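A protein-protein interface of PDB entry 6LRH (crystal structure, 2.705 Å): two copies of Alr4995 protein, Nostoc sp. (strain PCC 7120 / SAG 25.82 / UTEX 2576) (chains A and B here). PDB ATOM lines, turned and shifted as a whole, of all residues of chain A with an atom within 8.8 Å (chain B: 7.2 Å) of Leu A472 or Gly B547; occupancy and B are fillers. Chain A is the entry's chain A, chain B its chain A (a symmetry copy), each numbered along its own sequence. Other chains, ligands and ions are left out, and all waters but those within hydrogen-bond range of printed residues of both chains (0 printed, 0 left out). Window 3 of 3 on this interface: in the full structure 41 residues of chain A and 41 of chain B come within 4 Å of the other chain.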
ATOM      1  N   SER A 466      18.519 -20.881  -6.573  1.00  0.00           N
ATOM      2  CA  SER A 466      17.136 -20.512  -6.348  1.00  0.00           C
ATOM      3  C   SER A 466      16.790 -19.203  -7.053  1.00  0.00           C
ATOM      4  O   SER A 466      17.661 -18.498  -7.541  1.00  0.00           O
ATOM      5  CB  SER A 466      16.853 -20.407  -4.856  1.00  0.00           C
ATOM      6  OG  SER A 466      17.256 -19.155  -4.364  1.00  0.00           O
ATOM      7  N   GLU A 467      15.511 -18.886  -7.135  1.00  0.00           N
ATOM      8  CA  GLU A 467      15.117 -17.678  -7.837  1.00  0.00           C
ATOM      9  C   GLU A 467      15.559 -16.497  -7.035  1.00  0.00           C
ATOM     10  O   GLU A 467      15.997 -15.492  -7.575  1.00  0.00           O
ATOM     11  CB  GLU A 467      13.613 -17.622  -8.055  1.00  0.00           C
ATOM     12  CG  GLU A 467      13.139 -16.350  -8.701  1.00  0.00           C
ATOM     13  CD  GLU A 467      11.796 -15.933  -8.172  1.00  0.00           C
ATOM     14  OE1 GLU A 467      11.334 -14.817  -8.487  1.00  0.00           O
ATOM     15  OE2 GLU A 467      11.204 -16.728  -7.425  1.00  0.00           O
ATOM     16  N   ARG A 468      15.436 -16.645  -5.727  1.00  0.00           N
ATOM     17  CA  ARG A 468      15.754 -15.590  -4.797  1.00  0.00           C
ATOM     18  C   ARG A 468      17.221 -15.188  -4.923  1.00  0.00           C
ATOM     19  O   ARG A 468      17.544 -14.010  -4.876  1.00  0.00           O
ATOM     20  CB  ARG A 468      15.418 -16.038  -3.375  1.00  0.00           C
ATOM     21  CG  ARG A 468      15.694 -14.995  -2.326  1.00  0.00           C
ATOM     22  CD  ARG A 468      14.928 -13.724  -2.638  1.00  0.00           C
ATOM     23  NE  ARG A 468      15.170 -12.676  -1.651  1.00  0.00           N
ATOM     24  CZ  ARG A 468      14.897 -11.392  -1.856  1.00  0.00           C
ATOM     25  NH1 ARG A 468      15.140 -10.488  -0.913  1.00  0.00           N
ATOM     26  NH2 ARG A 468      14.380 -11.014  -3.017  1.00  0.00           N
ATOM     27  N   ARG A 469      18.103 -16.161  -5.127  1.00  0.00           N
ATOM     28  CA  ARG A 469      19.523 -15.856  -5.210  1.00  0.00           C
ATOM     29  C   ARG A 469      19.932 -15.250  -6.537  1.00  0.00           C
ATOM     30  O   ARG A 469      20.756 -14.350  -6.569  1.00  0.00           O
ATOM     31  CB  ARG A 469      20.391 -17.089  -4.956  1.00  0.00           C
ATOM     32  CG  ARG A 469      21.867 -16.701  -4.970  1.00  0.00           C
ATOM     33  CD  ARG A 469      22.856 -17.787  -4.613  1.00  0.00           C
ATOM     34  NE  ARG A 469      24.227 -17.271  -4.646  1.00  0.00           N
ATOM     35  CZ  ARG A 469      24.787 -16.562  -3.664  1.00  0.00           C
ATOM     36  NH1 ARG A 469      24.091 -16.266  -2.567  1.00  0.00           N
ATOM     37  NH2 ARG A 469      26.040 -16.138  -3.780  1.00  0.00           N
ATOM     38  N   VAL A 470      19.386 -15.745  -7.635  1.00  0.00           N
ATOM     39  CA  VAL A 470      19.778 -15.205  -8.928  1.00  0.00           C
ATOM     40  C   VAL A 470      19.367 -13.753  -8.998  1.00  0.00           C
ATOM     41  O   VAL A 470      20.061 -12.956  -9.583  1.00  0.00           O
ATOM     42  CB  VAL A 470      19.172 -15.986 -10.123  1.00  0.00           C
ATOM     43  CG1 VAL A 470      19.682 -17.412 -10.137  1.00  0.00           C
ATOM     44  CG2 VAL A 470      17.682 -15.980 -10.062  1.00  0.00           C
ATOM     45  N   GLU A 471      18.263 -13.396  -8.366  1.00  0.00           N
ATOM     46  CA  GLU A 471      17.826 -12.013  -8.403  1.00  0.00           C
ATOM     47  C   GLU A 471      18.734 -11.107  -7.572  1.00  0.00           C
ATOM     48  O   GLU A 471      19.106 -10.017  -8.007  1.00  0.00           O
ATOM     49  CB  GLU A 471      16.384 -11.902  -7.928  1.00  0.00           C
ATOM     50  CG  GLU A 471      15.394 -12.038  -9.043  1.00  0.00           C
ATOM     51  CD  GLU A 471      14.065 -12.580  -8.581  1.00  0.00           C
ATOM     52  OE1 GLU A 471      13.795 -12.537  -7.359  1.00  0.00           O
ATOM     53  OE2 GLU A 471      13.299 -13.062  -9.442  1.00  0.00           O
ATOM     54  N   LEU A 472      19.085 -11.571  -6.380  1.00  0.00           N
ATOM     55  CA  LEU A 472      19.987 -10.846  -5.503  1.00  0.00           C
ATOM     56  C   LEU A 472      21.349 -10.638  -6.139  1.00  0.00           C
ATOM     57  O   LEU A 472      21.916  -9.572  -6.013  1.00  0.00           O
ATOM     58  CB  LEU A 472      20.135 -11.573  -4.169  1.00  0.00           C
ATOM     59  CG  LEU A 472      18.950 -11.427  -3.215  1.00  0.00           C
ATOM     60  CD1 LEU A 472      19.153 -12.290  -1.998  1.00  0.00           C
ATOM     61  CD2 LEU A 472      18.735  -9.982  -2.806  1.00  0.00           C
ATOM     62  N   VAL A 473      21.877 -11.643  -6.819  1.00  0.00           N
ATOM     63  CA  VAL A 473      23.160 -11.497  -7.486  1.00  0.00           C
ATOM     64  C   VAL A 473      23.039 -10.564  -8.695  1.00  0.00           C
ATOM     65  O   VAL A 473      23.957  -9.821  -9.014  1.00  0.00           O
ATOM     66  CB  VAL A 473      23.724 -12.874  -7.926  1.00  0.00           C
ATOM     67  CG1 VAL A 473      24.904 -12.718  -8.853  1.00  0.00           C
ATOM     68  CG2 VAL A 473      24.112 -13.676  -6.728  1.00  0.00           C
ATOM     69  N   VAL A 474      21.900 -10.595  -9.366  1.00  0.00           N
ATOM     70  CA  VAL A 474      21.679  -9.713 -10.504  1.00  0.00           C
ATOM     71  C   VAL A 474      21.626  -8.264 -10.027  1.00  0.00           C
ATOM     72  O   VAL A 474      22.132  -7.375 -10.695  1.00  0.00           O
ATOM     73  CB  VAL A 474      20.389 -10.096 -11.267  1.00  0.00           C
ATOM     74  CG1 VAL A 474      19.892  -8.953 -12.127  1.00  0.00           C
ATOM     75  CG2 VAL A 474      20.626 -11.331 -12.108  1.00  0.00           C
ATOM     76  N   GLU A 475      21.034  -8.038  -8.857  1.00  0.00           N
ATOM     77  CA  GLU A 475      21.077  -6.735  -8.194  1.00  0.00           C
ATOM     78  C   GLU A 475      22.506  -6.243  -7.959  1.00  0.00           C
ATOM     79  O   GLU A 475      22.873  -5.149  -8.370  1.00  0.00           O
ATOM     80  CB  GLU A 475      20.347  -6.791  -6.853  1.00  0.00           C
ATOM     81  CG  GLU A 475      18.864  -6.532  -6.924  1.00  0.00           C
ATOM     82  CD  GLU A 475      18.228  -6.424  -5.549  1.00  0.00           C
ATOM     83  OE1 GLU A 475      18.935  -6.665  -4.545  1.00  0.00           O
ATOM     84  OE2 GLU A 475      17.028  -6.076  -5.469  1.00  0.00           O
ATOM     85  N   GLN A 476      23.299  -7.066  -7.287  1.00  0.00           N
ATOM     86  CA  GLN A 476      24.686  -6.761  -6.995  1.00  0.00           C
ATOM     87  C   GLN A 476      25.538  -6.507  -8.232  1.00  0.00           C
ATOM     88  O   GLN A 476      26.173  -5.476  -8.334  1.00  0.00           O
ATOM     89  CB  GLN A 476      25.303  -7.892  -6.177  1.00  0.00           C
ATOM     90  CG  GLN A 476      24.523  -8.227  -4.913  1.00  0.00           C
ATOM     91  CD  GLN A 476      24.714  -7.228  -3.780  1.00  0.00           C
ATOM     92  OE1 GLN A 476      24.729  -6.022  -3.989  1.00  0.00           O
ATOM     93  NE2 GLN A 476      24.830  -7.740  -2.563  1.00  0.00           N
ATOM     94  N   VAL A 477      25.569  -7.446  -9.163  1.00  0.00           N
ATOM     95  CA  VAL A 477      26.444  -7.324 -10.322  1.00  0.00           C
ATOM     96  C   VAL A 477      26.067  -6.121 -11.190  1.00  0.00           C
ATOM     97  O   VAL A 477      26.930  -5.438 -11.719  1.00  0.00           O
ATOM     98  CB  VAL A 477      26.429  -8.628 -11.161  1.00  0.00           C
ATOM     99  CG1 VAL A 477      27.265  -8.489 -12.422  1.00  0.00           C
ATOM    100  CG2 VAL A 477      26.941  -9.788 -10.327  1.00  0.00           C
ATOM    101  N   ALA A 478      24.773  -5.858 -11.314  1.00  0.00           N
ATOM    102  CA  ALA A 478      24.279  -4.709 -12.062  1.00  0.00           C
ATOM    103  C   ALA A 478      24.734  -3.404 -11.439  1.00  0.00           C
ATOM    104  O   ALA A 478      25.257  -2.530 -12.119  1.00  0.00           O
ATOM    105  CB  ALA A 478      22.780  -4.746 -12.144  1.00  0.00           C
ATOM    106  N   TRP A 479      24.522  -3.283 -10.138  1.00  0.00           N
ATOM    107  CA  TRP A 479      25.004  -2.154  -9.368  1.00  0.00           C
ATOM    108  C   TRP A 479      26.511  -1.943  -9.534  1.00  0.00           C
ATOM    109  O   TRP A 479      26.984  -0.813  -9.601  1.00  0.00           O
ATOM    110  CB  TRP A 479      24.649  -2.344  -7.894  1.00  0.00           C
ATOM    111  CG  TRP A 479      25.215  -1.302  -7.030  1.00  0.00           C
ATOM    112  CD1 TRP A 479      24.714  -0.064  -6.812  1.00  0.00           C
ATOM    113  CD2 TRP A 479      26.411  -1.391  -6.264  1.00  0.00           C
ATOM    114  NE1 TRP A 479      25.520   0.624  -5.954  1.00  0.00           N
ATOM    115  CE2 TRP A 479      26.574  -0.168  -5.607  1.00  0.00           C
ATOM    116  CE3 TRP A 479      27.360  -2.394  -6.064  1.00  0.00           C
ATOM    117  CZ2 TRP A 479      27.646   0.083  -4.767  1.00  0.00           C
ATOM    118  CZ3 TRP A 479      28.420  -2.143  -5.246  1.00  0.00           C
ATOM    119  CH2 TRP A 479      28.557  -0.916  -4.600  1.00  0.00           C
ATOM    120  N   VAL A 674      31.714 -14.221  -6.733  1.00  0.00           N
ATOM    121  CA  VAL A 674      30.348 -14.718  -6.633  1.00  0.00           C
ATOM    122  C   VAL A 674      30.019 -15.678  -7.790  1.00  0.00           C
ATOM    123  O   VAL A 674      30.406 -15.450  -8.931  1.00  0.00           O
ATOM    124  CB  VAL A 674      29.351 -13.533  -6.587  1.00  0.00           C
ATOM    125  CG1 VAL A 674      29.683 -12.520  -7.638  1.00  0.00           C
ATOM    126  CG2 VAL A 674      27.921 -14.001  -6.724  1.00  0.00           C
ATOM    127  N   VAL A 676      26.959 -18.126  -9.767  1.00  0.00           N
ATOM    128  CA  VAL A 676      25.528 -18.365  -9.931  1.00  0.00           C
ATOM    129  C   VAL A 676      25.276 -19.500 -10.938  1.00  0.00           C
ATOM    130  O   VAL A 676      25.903 -19.578 -11.990  1.00  0.00           O
ATOM    131  CB  VAL A 676      24.786 -17.058 -10.343  1.00  0.00           C
ATOM    132  CG1 VAL A 676      25.746 -15.898 -10.419  1.00  0.00           C
ATOM    133  CG2 VAL A 676      24.090 -17.203 -11.644  1.00  0.00           C
ATOM    134  N   PHE A 683      20.463 -15.208 -17.261  1.00  0.00           N
ATOM    135  CA  PHE A 683      21.209 -14.285 -16.454  1.00  0.00           C
ATOM    136  C   PHE A 683      21.375 -12.962 -17.194  1.00  0.00           C
ATOM    137  O   PHE A 683      21.058 -11.908 -16.661  1.00  0.00           O
ATOM    138  CB  PHE A 683      22.563 -14.892 -16.097  1.00  0.00           C
ATOM    139  CG  PHE A 683      23.411 -14.010 -15.240  1.00  0.00           C
ATOM    140  CD1 PHE A 683      23.124 -13.847 -13.902  1.00  0.00           C
ATOM    141  CD2 PHE A 683      24.497 -13.344 -15.772  1.00  0.00           C
ATOM    142  CE1 PHE A 683      23.893 -13.032 -13.124  1.00  0.00           C
ATOM    143  CE2 PHE A 683      25.272 -12.535 -14.992  1.00  0.00           C
ATOM    144  CZ  PHE A 683      24.969 -12.374 -13.670  1.00  0.00           C
ATOM    145  N   LEU A 686      18.099 -10.869 -17.435  1.00  0.00           N
ATOM    146  CA  LEU A 686      17.786 -10.173 -16.192  1.00  0.00           C
ATOM    147  C   LEU A 686      18.780  -9.068 -15.870  1.00  0.00           C
ATOM    148  O   LEU A 686      18.474  -8.124 -15.156  1.00  0.00           O
ATOM    149  CB  LEU A 686      17.763 -11.158 -15.028  1.00  0.00           C
ATOM    150  CG  LEU A 686      16.714 -12.248 -14.987  1.00  0.00           C
ATOM    151  CD1 LEU A 686      17.027 -13.202 -13.888  1.00  0.00           C
ATOM    152  CD2 LEU A 686      15.384 -11.644 -14.755  1.00  0.00           C
ATOM    153  N   GLN A 690      17.836  -5.274 -15.358  1.00  0.00           N
ATOM    154  CA  GLN A 690      18.155  -4.601 -14.110  1.00  0.00           C
ATOM    155  C   GLN A 690      18.948  -3.322 -14.331  1.00  0.00           C
ATOM    156  O   GLN A 690      18.791  -2.348 -13.597  1.00  0.00           O
ATOM    157  CB  GLN A 690      18.921  -5.534 -13.191  1.00  0.00           C
ATOM    158  CG  GLN A 690      19.242  -4.945 -11.834  1.00  0.00           C
ATOM    159  CD  GLN A 690      18.023  -4.761 -10.953  1.00  0.00           C
ATOM    160  OE1 GLN A 690      16.919  -5.171 -11.304  1.00  0.00           O
ATOM    161  NE2 GLN A 690      18.218  -4.132  -9.806  1.00  0.00           N
ATOM    162  N   ASP B 163      22.535  -5.731   4.003  1.00  0.00           N
ATOM    163  CA  ASP B 163      23.090  -5.426   2.689  1.00  0.00           C
ATOM    164  C   ASP B 163      24.334  -4.552   2.870  1.00  0.00           C
ATOM    165  O   ASP B 163      24.258  -3.461   3.424  1.00  0.00           O
ATOM    166  CB  ASP B 163      22.036  -4.713   1.836  1.00  0.00           C
ATOM    167  CG  ASP B 163      22.443  -4.549   0.384  1.00  0.00           C
ATOM    168  OD1 ASP B 163      21.545  -4.505  -0.479  1.00  0.00           O
ATOM    169  OD2 ASP B 163      23.649  -4.456   0.091  1.00  0.00           O
ATOM    170  N   ARG B 165      25.963  -2.690   0.997  1.00  0.00           N
ATOM    171  CA  ARG B 165      25.941  -1.400   0.333  1.00  0.00           C
ATOM    172  C   ARG B 165      25.244  -0.382   1.212  1.00  0.00           C
ATOM    173  O   ARG B 165      25.407   0.815   1.041  1.00  0.00           O
ATOM    174  CB  ARG B 165      25.227  -1.488  -1.001  1.00  0.00           C
ATOM    175  CG  ARG B 165      25.877  -2.370  -2.033  1.00  0.00           C
ATOM    176  CD  ARG B 165      24.956  -2.463  -3.193  1.00  0.00           C
ATOM    177  NE  ARG B 165      23.653  -2.943  -2.760  1.00  0.00           N
ATOM    178  CZ  ARG B 165      22.576  -2.959  -3.524  1.00  0.00           C
ATOM    179  NH1 ARG B 165      22.638  -2.504  -4.758  1.00  0.00           N
ATOM    180  NH2 ARG B 165      21.441  -3.420  -3.040  1.00  0.00           N
ATOM    181  N   GLY B 186      14.685  -3.592   1.771  1.00  0.00           N
ATOM    182  CA  GLY B 186      15.622  -4.619   1.357  1.00  0.00           C
ATOM    183  C   GLY B 186      16.941  -4.636   2.104  1.00  0.00           C
ATOM    184  O   GLY B 186      17.774  -5.506   1.889  1.00  0.00           O
ATOM    185  N   GLU B 210      14.708   0.118  -5.304  1.00  0.00           N
ATOM    186  CA  GLU B 210      16.155   0.037  -5.361  1.00  0.00           C
ATOM    187  C   GLU B 210      16.801   1.099  -6.254  1.00  0.00           C
ATOM    188  O   GLU B 210      17.901   1.576  -5.960  1.00  0.00           O
ATOM    189  CB  GLU B 210      16.603  -1.338  -5.821  1.00  0.00           C
ATOM    190  CG  GLU B 210      18.107  -1.447  -5.845  1.00  0.00           C
ATOM    191  CD  GLU B 210      18.596  -2.811  -6.181  1.00  0.00           C
ATOM    192  OE1 GLU B 210      17.771  -3.617  -6.648  1.00  0.00           O
ATOM    193  OE2 GLU B 210      19.803  -3.078  -5.989  1.00  0.00           O
ATOM    194  N   VAL B 542      14.848 -19.991   7.126  1.00  0.00           N
ATOM    195  CA  VAL B 542      15.692 -19.155   6.287  1.00  0.00           C
ATOM    196  C   VAL B 542      14.985 -17.867   5.891  1.00  0.00           C
ATOM    197  O   VAL B 542      13.998 -17.887   5.170  1.00  0.00           O
ATOM    198  CB  VAL B 542      16.126 -19.885   5.007  1.00  0.00           C
ATOM    199  CG1 VAL B 542      17.132 -19.048   4.255  1.00  0.00           C
ATOM    200  CG2 VAL B 542      16.695 -21.258   5.338  1.00  0.00           C
ATOM    201  N   ASP B 543      15.504 -16.753   6.386  1.00  0.00           N
ATOM    202  CA  ASP B 543      15.010 -15.425   6.052  1.00  0.00           C
ATOM    203  C   ASP B 543      14.936 -15.270   4.532  1.00  0.00           C
ATOM    204  O   ASP B 543      15.858 -15.648   3.838  1.00  0.00           O
ATOM    205  CB  ASP B 543      15.934 -14.364   6.668  1.00  0.00           C
ATOM    206  CG  ASP B 543      15.233 -13.056   6.936  1.00  0.00           C
ATOM    207  OD1 ASP B 543      14.901 -12.353   5.966  1.00  0.00           O
ATOM    208  OD2 ASP B 543      15.036 -12.714   8.113  1.00  0.00           O
ATOM    209  N   MET B 544      13.843 -14.733   4.012  1.00  0.00           N
ATOM    210  CA  MET B 544      13.721 -14.572   2.570  1.00  0.00           C
ATOM    211  C   MET B 544      14.348 -13.270   2.038  1.00  0.00           C
ATOM    212  O   MET B 544      14.627 -13.162   0.847  1.00  0.00           O
ATOM    213  CB  MET B 544      12.254 -14.639   2.157  1.00  0.00           C
ATOM    214  CG  MET B 544      12.038 -15.337   0.819  1.00  0.00           C
ATOM    215  SD  MET B 544      12.092 -17.137   0.943  1.00  0.00           S
ATOM    216  CE  MET B 544      10.483 -17.451   1.651  1.00  0.00           C
ATOM    217  N   LYS B 545      14.566 -12.289   2.917  1.00  0.00           N
ATOM    218  CA  LYS B 545      15.232 -11.038   2.549  1.00  0.00           C
ATOM    219  C   LYS B 545      16.688 -11.293   2.184  1.00  0.00           C
ATOM    220  O   LYS B 545      17.323 -10.521   1.470  1.00  0.00           O
ATOM    221  CB  LYS B 545      15.151 -10.022   3.694  1.00  0.00           C
ATOM    222  CG  LYS B 545      13.830  -9.269   3.800  1.00  0.00           C
ATOM    223  CD  LYS B 545      13.719  -8.206   2.718  1.00  0.00           C
ATOM    224  CE  LYS B 545      12.319  -7.619   2.633  1.00  0.00           C
ATOM    225  NZ  LYS B 545      12.044  -7.070   1.265  1.00  0.00           N
ATOM    226  N   ARG B 546      17.209 -12.386   2.717  1.00  0.00           N
ATOM    227  CA  ARG B 546      18.542 -12.862   2.397  1.00  0.00           C
ATOM    228  C   ARG B 546      18.351 -14.185   1.681  1.00  0.00           C
ATOM    229  O   ARG B 546      17.331 -14.826   1.849  1.00  0.00           O
ATOM    230  CB  ARG B 546      19.376 -13.012   3.671  1.00  0.00           C
ATOM    231  CG  ARG B 546      19.129 -11.884   4.687  1.00  0.00           C
ATOM    232  CD  ARG B 546      19.493 -12.264   6.120  1.00  0.00           C
ATOM    233  NE  ARG B 546      20.846 -12.789   6.197  1.00  0.00           N
ATOM    234  CZ  ARG B 546      21.325 -13.451   7.239  1.00  0.00           C
ATOM    235  NH1 ARG B 546      20.554 -13.663   8.295  1.00  0.00           N
ATOM    236  NH2 ARG B 546      22.571 -13.907   7.221  1.00  0.00           N
ATOM    237  N   GLY B 547      19.296 -14.601   0.859  1.00  0.00           N
ATOM    238  CA  GLY B 547      19.125 -15.871   0.183  1.00  0.00           C
ATOM    239  C   GLY B 547      19.672 -17.022   1.003  1.00  0.00           C
ATOM    240  O   GLY B 547      19.708 -18.160   0.545  1.00  0.00           O
ATOM    241  N   VAL B 548      20.090 -16.725   2.230  1.00  0.00           N
ATOM    242  CA  VAL B 548      20.964 -17.626   2.973  1.00  0.00           C
ATOM    243  C   VAL B 548      20.633 -17.788   4.452  1.00  0.00           C
ATOM    244  O   VAL B 548      19.883 -17.004   5.026  1.00  0.00           O
ATOM    245  CB  VAL B 548      22.423 -17.146   2.881  1.00  0.00           C
ATOM    246  CG1 VAL B 548      22.948 -17.276   1.454  1.00  0.00           C
ATOM    247  CG2 VAL B 548      22.530 -15.702   3.376  1.00  0.00           C
ATOM    248  N   ALA B 549      21.218 -18.821   5.050  1.00  0.00           N
ATOM    249  CA  ALA B 549      21.249 -18.996   6.498  1.00  0.00           C
ATOM    250  C   ALA B 549      22.371 -19.963   6.848  1.00  0.00           C
ATOM    251  O   ALA B 549      22.587 -20.932   6.126  1.00  0.00           O
ATOM    252  CB  ALA B 549      19.920 -19.508   7.020  1.00  0.00           C
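No position is printed for both chains.
Of the 7 pairs that touch across the chains among the printed residues, none has its exchanged pair printed and touching as well.
Of chain B, only Gly B547 (3.7 Å) comes within 4 Å of Leu A472.
Printed residues of chain A within 4 Å of Gly B547: Leu A472 (3.7 Å).
No residue of chain A comes within 4 Å of Val B548.
Of the printed residues of chain B, Gln A690 touches Glu B210 (3.2 Å).
Of the printed residues of chain B, Glu A475 touches Glu B210.
Of the printed residues of chain A, Glu B210 touches Glu A475 (2.8 Å) and Gln A690 (3.2 Å).
Of the printed residues of chain A, Arg B165 touches Gln A476 and Trp A479.
Val A473 touches none of the printed residues of chain B.
The nearest printed residue of chain A that does not touch Arg B165 is Glu A475 (4.4 Å).
NE of Arg A468 sits at hydrogen-bond distance from O of Met B544 (2.6 Å).
The guanidinium group (NH1) of Arg A468 lies within hydrogen-bond range of the backbone carbonyl oxygen (O) of Lys B545, at 3.2 Å.
OE1 of Gln A476 sits at hydrogen-bond distance from NE of Arg B165, at 3.5 Å.
The side-chain amide nitrogen (NE2) of Gln A690 is in hydrogen-bond range of the side-chain carboxylate (OE1) of Glu B210 (3.2 Å).
The side-chain carboxylate (OE1) of Glu B210 sits close to the side-chain carboxylate (OE2) of Glu A475, at 2.8 Å.
N of Arg A468 sits close to OG of Ser A466 (3.4 Å).
The guanidinium group of Arg B165 lies within salt-bridge range of the side-chain carboxylate of Asp B163 (2.8 Å).
The guanidinium group (NH1) of Arg B165 lies within salt-bridge range of the side-chain carboxylate (OE2) of Glu B210 (3.1 Å).
The side-chain carboxylate (OD1) of Asp B543 is in hydrogen-bond range of the backbone NH (N) of Lys B545, at 3.1 Å.
Leu A472 touches Gly B547.
Trp A479 touches Arg B165.
Printed residues of chain A that touch a printed residue of chain B: Arg A468, Leu A472, Glu A475, Gln A476, Trp A479 and Gln A690.
Hydrophobic or aromatic side chains of chain A that line the printed part of chain B: Leu A472 and Trp A479.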
